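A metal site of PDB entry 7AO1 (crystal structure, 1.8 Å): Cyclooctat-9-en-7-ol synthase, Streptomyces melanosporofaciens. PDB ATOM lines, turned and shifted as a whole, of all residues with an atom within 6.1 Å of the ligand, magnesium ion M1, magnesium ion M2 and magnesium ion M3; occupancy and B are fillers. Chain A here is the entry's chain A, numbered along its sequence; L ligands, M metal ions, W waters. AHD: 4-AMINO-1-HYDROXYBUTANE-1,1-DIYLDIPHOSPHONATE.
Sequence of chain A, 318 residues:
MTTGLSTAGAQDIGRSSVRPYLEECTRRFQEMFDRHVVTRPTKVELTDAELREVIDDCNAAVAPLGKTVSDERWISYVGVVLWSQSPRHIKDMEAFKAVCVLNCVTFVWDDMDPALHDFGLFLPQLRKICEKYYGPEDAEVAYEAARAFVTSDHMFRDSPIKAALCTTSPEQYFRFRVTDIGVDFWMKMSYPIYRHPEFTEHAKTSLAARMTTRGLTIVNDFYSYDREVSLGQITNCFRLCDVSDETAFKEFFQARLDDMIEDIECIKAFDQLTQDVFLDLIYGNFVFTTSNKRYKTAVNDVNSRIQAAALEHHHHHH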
ATOM      1  N   ASN A 103      21.506  -4.636   7.226  1.00  0.00           N
ATOM      2  CA  ASN A 103      20.933  -3.537   6.473  1.00  0.00           C
ATOM      3  C   ASN A 103      20.093  -2.626   7.369  1.00  0.00           C
ATOM      4  O   ASN A 103      20.203  -1.401   7.270  1.00  0.00           O
ATOM      5  CB  ASN A 103      20.104  -4.067   5.306  1.00  0.00           C
ATOM      6  CG  ASN A 103      20.039  -3.093   4.168  1.00  0.00           C
ATOM      7  OD1 ASN A 103      18.989  -2.506   3.909  1.00  0.00           O
ATOM      8  ND2 ASN A 103      21.204  -2.863   3.527  1.00  0.00           N
ATOM      9  N   THR A 106      22.378  -0.455   9.677  1.00  0.00           N
ATOM     10  CA  THR A 106      23.096   0.587   8.923  1.00  0.00           C
ATOM     11  C   THR A 106      22.155   1.630   8.295  1.00  0.00           C
ATOM     12  O   THR A 106      22.585   2.749   8.031  1.00  0.00           O
ATOM     13  CB  THR A 106      24.032  -0.055   7.863  1.00  0.00           C
ATOM     14  OG1 THR A 106      23.298  -0.921   6.987  1.00  0.00           O
ATOM     15  CG2 THR A 106      25.102  -0.860   8.544  1.00  0.00           C
ATOM     16  N   PHE A 107      20.867   1.307   8.092  1.00  0.00           N
ATOM     17  CA  PHE A 107      19.869   2.337   7.791  1.00  0.00           C
ATOM     18  C   PHE A 107      19.771   3.343   8.929  1.00  0.00           C
ATOM     19  O   PHE A 107      19.724   4.557   8.705  1.00  0.00           O
ATOM     20  CB  PHE A 107      18.527   1.669   7.570  1.00  0.00           C
ATOM     21  CG  PHE A 107      18.008   1.775   6.184  1.00  0.00           C
ATOM     22  CD1 PHE A 107      17.698   3.025   5.633  1.00  0.00           C
ATOM     23  CD2 PHE A 107      17.782   0.640   5.436  1.00  0.00           C
ATOM     24  CE1 PHE A 107      17.216   3.111   4.378  1.00  0.00           C
ATOM     25  CE2 PHE A 107      17.284   0.727   4.168  1.00  0.00           C
ATOM     26  CZ  PHE A 107      16.992   1.955   3.641  1.00  0.00           C
ATOM     27  N   ASP A 110      22.567   5.589   8.701  1.00  0.00           N
ATOM     28  CA  ASP A 110      22.382   6.518   7.586  1.00  0.00           C
ATOM     29  C   ASP A 110      21.466   7.668   7.987  1.00  0.00           C
ATOM     30  O   ASP A 110      21.616   8.791   7.482  1.00  0.00           O
ATOM     31  CB  ASP A 110      21.759   5.753   6.378  1.00  0.00           C
ATOM     32  CG  ASP A 110      21.629   6.606   5.112  1.00  0.00           C
ATOM     33  OD1 ASP A 110      22.679   6.846   4.407  1.00  0.00           O
ATOM     34  OD2 ASP A 110      20.475   7.019   4.771  1.00  0.00           O
ATOM     35  N   ASP A 111      20.528   7.386   8.872  1.00  0.00           N
ATOM     36  CA  ASP A 111      19.520   8.363   9.289  1.00  0.00           C
ATOM     37  C   ASP A 111      19.944   9.197  10.490  1.00  0.00           C
ATOM     38  O   ASP A 111      19.159  10.026  10.946  1.00  0.00           O
ATOM     39  CB  ASP A 111      18.217   7.620   9.627  1.00  0.00           C
ATOM     40  CG  ASP A 111      17.370   7.380   8.423  1.00  0.00           C
ATOM     41  OD1 ASP A 111      17.632   8.007   7.399  1.00  0.00           O
ATOM     42  OD2 ASP A 111      16.423   6.564   8.506  1.00  0.00           O
ATOM     43  N   PHE A 149      31.095   0.623   4.911  1.00  0.00           N
ATOM     44  CA  PHE A 149      29.941   1.439   4.577  1.00  0.00           C
ATOM     45  C   PHE A 149      29.715   2.524   5.620  1.00  0.00           C
ATOM     46  O   PHE A 149      29.444   3.686   5.275  1.00  0.00           O
ATOM     47  CB  PHE A 149      28.678   0.586   4.446  1.00  0.00           C
ATOM     48  CG  PHE A 149      27.433   1.408   4.275  1.00  0.00           C
ATOM     49  CD1 PHE A 149      27.102   1.943   3.046  1.00  0.00           C
ATOM     50  CD2 PHE A 149      26.590   1.637   5.339  1.00  0.00           C
ATOM     51  CE1 PHE A 149      25.908   2.686   2.874  1.00  0.00           C
ATOM     52  CE2 PHE A 149      25.419   2.365   5.186  1.00  0.00           C
ATOM     53  CZ  PHE A 149      25.059   2.880   3.962  1.00  0.00           C
ATOM     54  N   ASP A 153      29.872   6.589   5.049  1.00  0.00           N
ATOM     55  CA  ASP A 153      28.750   7.475   5.334  1.00  0.00           C
ATOM     56  C   ASP A 153      29.148   8.553   6.348  1.00  0.00           C
ATOM     57  O   ASP A 153      28.677   9.692   6.271  1.00  0.00           O
ATOM     58  CB  ASP A 153      27.581   6.677   5.890  1.00  0.00           C
ATOM     59  CG  ASP A 153      26.477   7.587   6.378  1.00  0.00           C
ATOM     60  OD1 ASP A 153      25.954   8.343   5.555  1.00  0.00           O
ATOM     61  OD2 ASP A 153      26.153   7.554   7.587  1.00  0.00           O
ATOM     62  N   ARG A 177      28.389   6.567  -5.584  1.00  0.00           N
ATOM     63  CA  ARG A 177      27.294   5.794  -5.025  1.00  0.00           C
ATOM     64  C   ARG A 177      27.536   4.265  -5.021  1.00  0.00           C
ATOM     65  O   ARG A 177      26.857   3.554  -4.260  1.00  0.00           O
ATOM     66  CB  ARG A 177      26.027   6.094  -5.821  1.00  0.00           C
ATOM     67  CG  ARG A 177      25.555   7.566  -5.554  1.00  0.00           C
ATOM     68  CD  ARG A 177      25.059   7.658  -4.109  1.00  0.00           C
ATOM     69  NE  ARG A 177      23.591   7.834  -4.092  1.00  0.00           N
ATOM     70  CZ  ARG A 177      22.773   7.494  -3.071  1.00  0.00           C
ATOM     71  NH1 ARG A 177      23.254   6.987  -1.950  1.00  0.00           N
ATOM     72  NH2 ARG A 177      21.443   7.634  -3.195  1.00  0.00           N
ATOM     73  N   ASP A 180      28.449   4.466  -1.683  1.00  0.00           N
ATOM     74  CA  ASP A 180      27.691   5.263  -0.716  1.00  0.00           C
ATOM     75  C   ASP A 180      26.242   4.763  -0.542  1.00  0.00           C
ATOM     76  O   ASP A 180      25.708   4.785   0.579  1.00  0.00           O
ATOM     77  CB  ASP A 180      27.686   6.726  -1.116  1.00  0.00           C
ATOM     78  CG  ASP A 180      26.719   7.563  -0.271  1.00  0.00           C
ATOM     79  OD1 ASP A 180      27.088   7.923   0.863  1.00  0.00           O
ATOM     80  OD2 ASP A 180      25.565   7.789  -0.712  1.00  0.00           O
ATOM     81  N   ILE A 181      25.601   4.278  -1.624  1.00  0.00           N
ATOM     82  CA  ILE A 181      24.235   3.789  -1.475  1.00  0.00           C
ATOM     83  C   ILE A 181      24.232   2.476  -0.708  1.00  0.00           C
ATOM     84  O   ILE A 181      23.184   2.069  -0.202  1.00  0.00           O
ATOM     85  CB  ILE A 181      23.510   3.661  -2.831  1.00  0.00           C
ATOM     86  CG1 ILE A 181      21.962   3.688  -2.635  1.00  0.00           C
ATOM     87  CG2 ILE A 181      23.971   2.369  -3.595  1.00  0.00           C
ATOM     88  CD1 ILE A 181      21.209   3.918  -3.886  1.00  0.00           C
ATOM     89  N   GLY A 182      25.398   1.818  -0.580  1.00  0.00           N
ATOM     90  CA  GLY A 182      25.481   0.557   0.144  1.00  0.00           C
ATOM     91  C   GLY A 182      25.343  -0.689  -0.719  1.00  0.00           C
ATOM     92  O   GLY A 182      25.227  -1.805  -0.160  1.00  0.00           O
ATOM     93  N   ASN A 220      16.026   5.166  -6.279  1.00  0.00           N
ATOM     94  CA  ASN A 220      16.038   5.741  -4.950  1.00  0.00           C
ATOM     95  C   ASN A 220      16.085   7.259  -5.014  1.00  0.00           C
ATOM     96  O   ASN A 220      15.454   7.921  -4.192  1.00  0.00           O
ATOM     97  CB  ASN A 220      17.235   5.239  -4.119  1.00  0.00           C
ATOM     98  CG  ASN A 220      17.296   5.912  -2.738  1.00  0.00           C
ATOM     99  OD1 ASN A 220      17.984   6.920  -2.556  1.00  0.00           O
ATOM    100  ND2 ASN A 220      16.554   5.378  -1.783  1.00  0.00           N
ATOM    101  N   ASP A 221      16.903   7.813  -5.918  1.00  0.00           N
ATOM    102  CA  ASP A 221      17.101   9.271  -5.931  1.00  0.00           C
ATOM    103  C   ASP A 221      15.783   9.973  -6.254  1.00  0.00           C
ATOM    104  O   ASP A 221      15.439  11.016  -5.674  1.00  0.00           O
ATOM    105  CB  ASP A 221      18.168   9.667  -6.928  1.00  0.00           C
ATOM    106  CG  ASP A 221      19.612   9.433  -6.402  1.00  0.00           C
ATOM    107  OD1 ASP A 221      19.798   9.051  -5.214  1.00  0.00           O
ATOM    108  OD2 ASP A 221      20.543   9.618  -7.216  1.00  0.00           O
ATOM    109  N   SER A 224      13.491   9.752  -3.057  1.00  0.00           N
ATOM    110  CA  SER A 224      13.987  10.302  -1.822  1.00  0.00           C
ATOM    111  C   SER A 224      14.468  11.739  -2.015  1.00  0.00           C
ATOM    112  O   SER A 224      14.969  12.346  -1.059  1.00  0.00           O
ATOM    113  CB  SER A 224      15.096   9.415  -1.241  1.00  0.00           C
ATOM    114  OG  SER A 224      16.304   9.586  -1.969  1.00  0.00           O
ATOM    115  N   TYR A 225      14.305  12.305  -3.213  1.00  0.00           N
ATOM    116  CA  TYR A 225      14.695  13.680  -3.485  1.00  0.00           C
ATOM    117  C   TYR A 225      14.072  14.657  -2.491  1.00  0.00           C
ATOM    118  O   TYR A 225      14.765  15.504  -1.918  1.00  0.00           O
ATOM    119  CB  TYR A 225      14.293  14.079  -4.900  1.00  0.00           C
ATOM    120  CG  TYR A 225      14.670  15.473  -5.300  1.00  0.00           C
ATOM    121  CD1 TYR A 225      15.939  15.738  -5.797  1.00  0.00           C
ATOM    122  CD2 TYR A 225      13.751  16.538  -5.233  1.00  0.00           C
ATOM    123  CE1 TYR A 225      16.312  16.991  -6.194  1.00  0.00           C
ATOM    124  CE2 TYR A 225      14.121  17.797  -5.643  1.00  0.00           C
ATOM    125  CZ  TYR A 225      15.403  18.035  -6.109  1.00  0.00           C
ATOM    126  OH  TYR A 225      15.798  19.293  -6.534  1.00  0.00           O
ATOM    127  N   ARG A 227      12.658  14.418   0.519  1.00  0.00           N
ATOM    128  CA  ARG A 227      13.229  14.309   1.855  1.00  0.00           C
ATOM    129  C   ARG A 227      14.655  14.851   1.887  1.00  0.00           C
ATOM    130  O   ARG A 227      15.010  15.645   2.772  1.00  0.00           O
ATOM    131  CB  ARG A 227      13.200  12.842   2.329  1.00  0.00           C
ATOM    132  CG  ARG A 227      14.208  12.537   3.434  1.00  0.00           C
ATOM    133  CD  ARG A 227      13.898  11.256   4.217  1.00  0.00           C
ATOM    134  NE  ARG A 227      13.800  10.071   3.338  1.00  0.00           N
ATOM    135  CZ  ARG A 227      14.824   9.369   2.858  1.00  0.00           C
ATOM    136  NH1 ARG A 227      16.096   9.667   3.176  1.00  0.00           N
ATOM    137  NH2 ARG A 227      14.579   8.332   2.054  1.00  0.00           N
ATOM    138  N   GLU A 228      15.477  14.476   0.895  1.00  0.00           N
ATOM    139  CA  GLU A 228      16.895  14.820   0.966  1.00  0.00           C
ATOM    140  C   GLU A 228      17.130  16.315   0.763  1.00  0.00           C
ATOM    141  O   GLU A 228      17.951  16.913   1.477  1.00  0.00           O
ATOM    142  CB  GLU A 228      17.703  13.964  -0.032  1.00  0.00           C
ATOM    143  CG  GLU A 228      17.850  12.507   0.527  1.00  0.00           C
ATOM    144  CD  GLU A 228      18.287  11.458  -0.475  1.00  0.00           C
ATOM    145  OE1 GLU A 228      18.585  11.790  -1.647  1.00  0.00           O
ATOM    146  OE2 GLU A 228      18.341  10.305  -0.051  1.00  0.00           O
ATOM    147  N   GLN A 233      20.676  17.377   2.157  1.00  0.00           N
ATOM    148  CA  GLN A 233      21.515  16.270   1.676  1.00  0.00           C
ATOM    149  C   GLN A 233      21.749  16.405   0.164  1.00  0.00           C
ATOM    150  O   GLN A 233      20.798  16.489  -0.614  1.00  0.00           O
ATOM    151  CB  GLN A 233      20.843  14.934   2.047  1.00  0.00           C
ATOM    152  CG  GLN A 233      21.058  14.593   3.537  1.00  0.00           C
ATOM    153  CD  GLN A 233      20.171  13.495   4.069  1.00  0.00           C
ATOM    154  OE1 GLN A 233      18.997  13.434   3.744  1.00  0.00           O
ATOM    155  NE2 GLN A 233      20.734  12.618   4.903  1.00  0.00           N
ATOM    156  N   THR A 235      23.381  14.202  -1.911  1.00  0.00           N
ATOM    157  CA  THR A 235      23.682  12.917  -2.603  1.00  0.00           C
ATOM    158  C   THR A 235      22.429  12.453  -3.333  1.00  0.00           C
ATOM    159  O   THR A 235      21.656  11.612  -2.876  1.00  0.00           O
ATOM    160  CB  THR A 235      24.178  11.869  -1.607  1.00  0.00           C
ATOM    161  OG1 THR A 235      25.270  12.409  -0.882  1.00  0.00           O
ATOM    162  CG2 THR A 235      24.702  10.590  -2.321  1.00  0.00           C
ATOM    163  N   ASN A 236      22.232  12.992  -4.537  1.00  0.00           N
ATOM    164  CA  ASN A 236      21.031  12.674  -5.314  1.00  0.00           C
ATOM    165  C   ASN A 236      21.205  13.181  -6.728  1.00  0.00           C
ATOM    166  O   ASN A 236      21.421  14.394  -6.914  1.00  0.00           O
ATOM    167  CB  ASN A 236      19.796  13.323  -4.682  1.00  0.00           C
ATOM    168  CG  ASN A 236      18.537  12.910  -5.356  1.00  0.00           C
ATOM    169  OD1 ASN A 236      18.364  13.107  -6.597  1.00  0.00           O
ATOM    170  ND2 ASN A 236      17.636  12.313  -4.588  1.00  0.00           N
ATOM    171  N   ARG A 294       8.514   5.023   4.010  1.00  0.00           N
ATOM    172  CA  ARG A 294       9.736   5.811   4.031  1.00  0.00           C
ATOM    173  C   ARG A 294       9.759   6.847   2.913  1.00  0.00           C
ATOM    174  O   ARG A 294      10.218   7.968   3.079  1.00  0.00           O
ATOM    175  CB  ARG A 294      10.951   4.885   3.948  1.00  0.00           C
ATOM    176  CG  ARG A 294      12.304   5.632   3.884  1.00  0.00           C
ATOM    177  CD  ARG A 294      13.526   4.709   3.969  1.00  0.00           C
ATOM    178  NE  ARG A 294      14.801   5.446   3.971  1.00  0.00           N
ATOM    179  CZ  ARG A 294      15.309   6.076   5.031  1.00  0.00           C
ATOM    180  NH1 ARG A 294      14.645   6.067   6.185  1.00  0.00           N
ATOM    181  NH2 ARG A 294      16.472   6.729   4.930  1.00  0.00           N
ATOM    182  N   TYR A 295       9.274   6.468   1.733  1.00  0.00           N
ATOM    183  CA  TYR A 295       9.310   7.375   0.596  1.00  0.00           C
ATOM    184  C   TYR A 295       7.945   8.009   0.348  1.00  0.00           C
ATOM    185  O   TYR A 295       7.750   8.635  -0.697  1.00  0.00           O
ATOM    186  CB  TYR A 295       9.803   6.630  -0.648  1.00  0.00           C
ATOM    187  CG  TYR A 295      11.118   5.950  -0.338  1.00  0.00           C
ATOM    188  CD1 TYR A 295      12.316   6.696  -0.352  1.00  0.00           C
ATOM    189  CD2 TYR A 295      11.153   4.641   0.043  1.00  0.00           C
ATOM    190  CE1 TYR A 295      13.535   6.105  -0.015  1.00  0.00           C
ATOM    191  CE2 TYR A 295      12.370   4.022   0.381  1.00  0.00           C
ATOM    192  CZ  TYR A 295      13.558   4.775   0.349  1.00  0.00           C
ATOM    193  OH  TYR A 295      14.772   4.176   0.674  1.00  0.00           O
HETATM  194  C2  AHD L   1      20.424   3.632   1.705  1.00  0.00           C
HETATM  195  C3  AHD L   1      20.934   2.813   2.864  1.00  0.00           C
HETATM  196  C7  AHD L   1      19.512   4.750   2.245  1.00  0.00           C
HETATM  197  C8  AHD L   1      19.116   5.642   1.073  1.00  0.00           C
HETATM  198  O12 AHD L   1      18.071   7.504   2.710  1.00  0.00           O
HETATM  199  P9  AHD L   1      17.644   6.705   1.514  1.00  0.00           P
HETATM  200  O10 AHD L   1      17.302   7.559   0.288  1.00  0.00           O
HETATM  201  O11 AHD L   1      16.597   5.679   1.862  1.00  0.00           O
HETATM  202  P14 AHD L   1      20.506   6.788   0.585  1.00  0.00           P
HETATM  203  O15 AHD L   1      21.627   5.902  -0.053  1.00  0.00           O
HETATM  204  O16 AHD L   1      20.020   7.772  -0.409  1.00  0.00           O
HETATM  205  O17 AHD L   1      21.113   7.461   1.794  1.00  0.00           O
HETATM  206  O13 AHD L   1      18.814   4.827  -0.040  1.00  0.00           O
HETATM  207  N4  AHD L   1      21.170   1.451   2.413  1.00  0.00           N
HETATM  208 MG    MG M   1      18.195   8.466  -1.171  1.00  0.00          MG
HETATM  209 MG    MG M   2      19.873   8.307   3.271  1.00  0.00          MG
HETATM  210 MG    MG M   3      22.979   7.607   2.503  1.00  0.00          MG
HETATM  211  O   HOH W   1      17.207   2.747   0.158  1.00  0.00           O
HETATM  212  O   HOH W   2      19.276  10.046   2.351  1.00  0.00           O
HETATM  213  O   HOH W   3      18.996   9.232   5.033  1.00  0.00           O
HETATM  214  O   HOH W   4      23.332   5.718   1.799  1.00  0.00           O
HETATM  215  O   HOH W   5      19.114   9.426  -2.757  1.00  0.00           O
HETATM  216  O   HOH W   6      23.557   8.734   0.946  1.00  0.00           O
HETATM  217  O   HOH W   7      21.941   9.289   3.421  1.00  0.00           O
HETATM  218  O   HOH W   8      24.969   7.894   3.058  1.00  0.00           O
HETATM  219  O   HOH W   9      21.555   9.963  -0.498  1.00  0.00           O
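An oxygen (O12) of the ligand is bound to magnesium ion M2 (2.1 Å).
Water W2 binds magnesium ion M2.
OD2 of Asp 110 is bound to magnesium ion M2, at 2.1 Å.
O17 of the ligand is bound to magnesium ion M2 (2.1 Å).
Magnesium ion M2 is bound by water W3, at 2.2 Å.
Water W7 binds magnesium ion M2 (2.3 Å).
Magnesium ion M2 has six donor atoms within binding distance.
Phe 107 touches the ligand.
Hydrophobic or aromatic side chains that line the ligand: Phe 107, Ile 181 and Tyr 295.
Ten residues have an atom within 4 Å of the ligand: Phe 107, Asp 110, Arg 177, Ile 181, Asn 220, Ser 224, Arg 227, Glu 228, Arg 294 and Tyr 295.
The nearest printed residue that does not touch the ligand is Phe 149 (4.3 Å).
The side-chain hydroxyl (OH) of Tyr 295 is in hydrogen-bond range of an oxygen (O11) of the ligand, at 2.6 Å.
An oxygen (O15) of the ligand lies within salt-bridge range of the guanidinium group of Arg 177 (2.7 Å).
NE of Arg 294 is in salt-bridge range of O11 of the ligand, at 2.8 Å.
O11 of the ligand lies within salt-bridge range of NH2 of Arg 227, at 3.3 Å.
The backbone carbonyl oxygen of Ile 181 sits at hydrogen-bond distance from a nitrogen (N4) of the ligand, at 3.4 Å.
An oxygen (O17) of the ligand binds magnesium ion M3, at 2.0 Å.
Water W6 is bound to magnesium ion M3, 2.0 Å away.
Water W4 is bound to magnesium ion M3 (2.0 Å).
The side-chain carboxylate (OD1) of Asp 110 is bound to magnesium ion M3, at 2.1 Å.
Water W8 binds magnesium ion M3 (2.1 Å).
Water W7 is bound to magnesium ion M3, 2.2 Å away.
Magnesium ion M3 has six donor atoms within binding distance.
ND2 of Asn 220 lies within hydrogen-bond range of OH of Tyr 295 (3.3 Å).
OE2 of Glu 228 sits close to NH1 of Arg 227 (3.98 Å).
The backbone carbonyl oxygen (O) of Glu 228 is in hydrogen-bond range of the backbone NH (N) of Gln 233, at 2.8 Å.
The side-chain amide nitrogen of Asn 236 lies within hydrogen-bond range of the side-chain carboxylate of Glu 228, at 3.1 Å.
The side-chain carboxylate (OD2) of Asp 180 is in salt-bridge range of the guanidinium group (NH1) of Arg 177.
NH2 of Arg 177 lies within salt-bridge range of OD1 of Asp 221.
The side-chain carboxylate of Asp 111 is in salt-bridge range of the guanidinium group of Arg 294 (3.0 Å).
One residue has an atom within 4 Å of magnesium ion M2: Asp 110.
Of the 22 residues printed, 1 comes within 4 Å of magnesium ion M3.
The nearest printed residue that does not touch magnesium ion M3 is Asp 180 (4.1 Å).
Magnesium ion M1 is bound by an oxygen (O10) of the ligand (1.9 Å), water W5 (2.1 Å), the side-chain amide oxygen (OD1) of Asn 220 (2.1 Å), an oxygen (O16) of the ligand (2.1 Å), the side-chain carboxylate (OE2) of Glu 228 (2.2 Å) and the side-chain hydroxyl (OG) of Ser 224 (2.3 Å).
Water W3 bridges OD1 of Asp 111 (3.0 Å) and NH1 of Arg 227 (3.5 Å).
Water W4 lies within hydrogen-bond range of an oxygen (O15) of the ligand and the backbone carbonyl oxygen (O) of Asp 180.
Water W8 lies within hydrogen-bond range of the side-chain carboxylate of Asp 153 and the side-chain carboxylate of Asp 180.
Water W6 lies within hydrogen-bond range of OD2 of Asp 180 (2.8 Å) and NH1 of Arg 177 (3.4 Å).
Water W1 lies within hydrogen-bond range of O13 of the ligand (2.6 Å), OH of Tyr 295 (2.9 Å) and ND2 of Asn 220 (3.3 Å).
Arg 177 touches magnesium ion M1.
Of the 22 residues printed, 4 come within 4 Å of magnesium ion M1.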
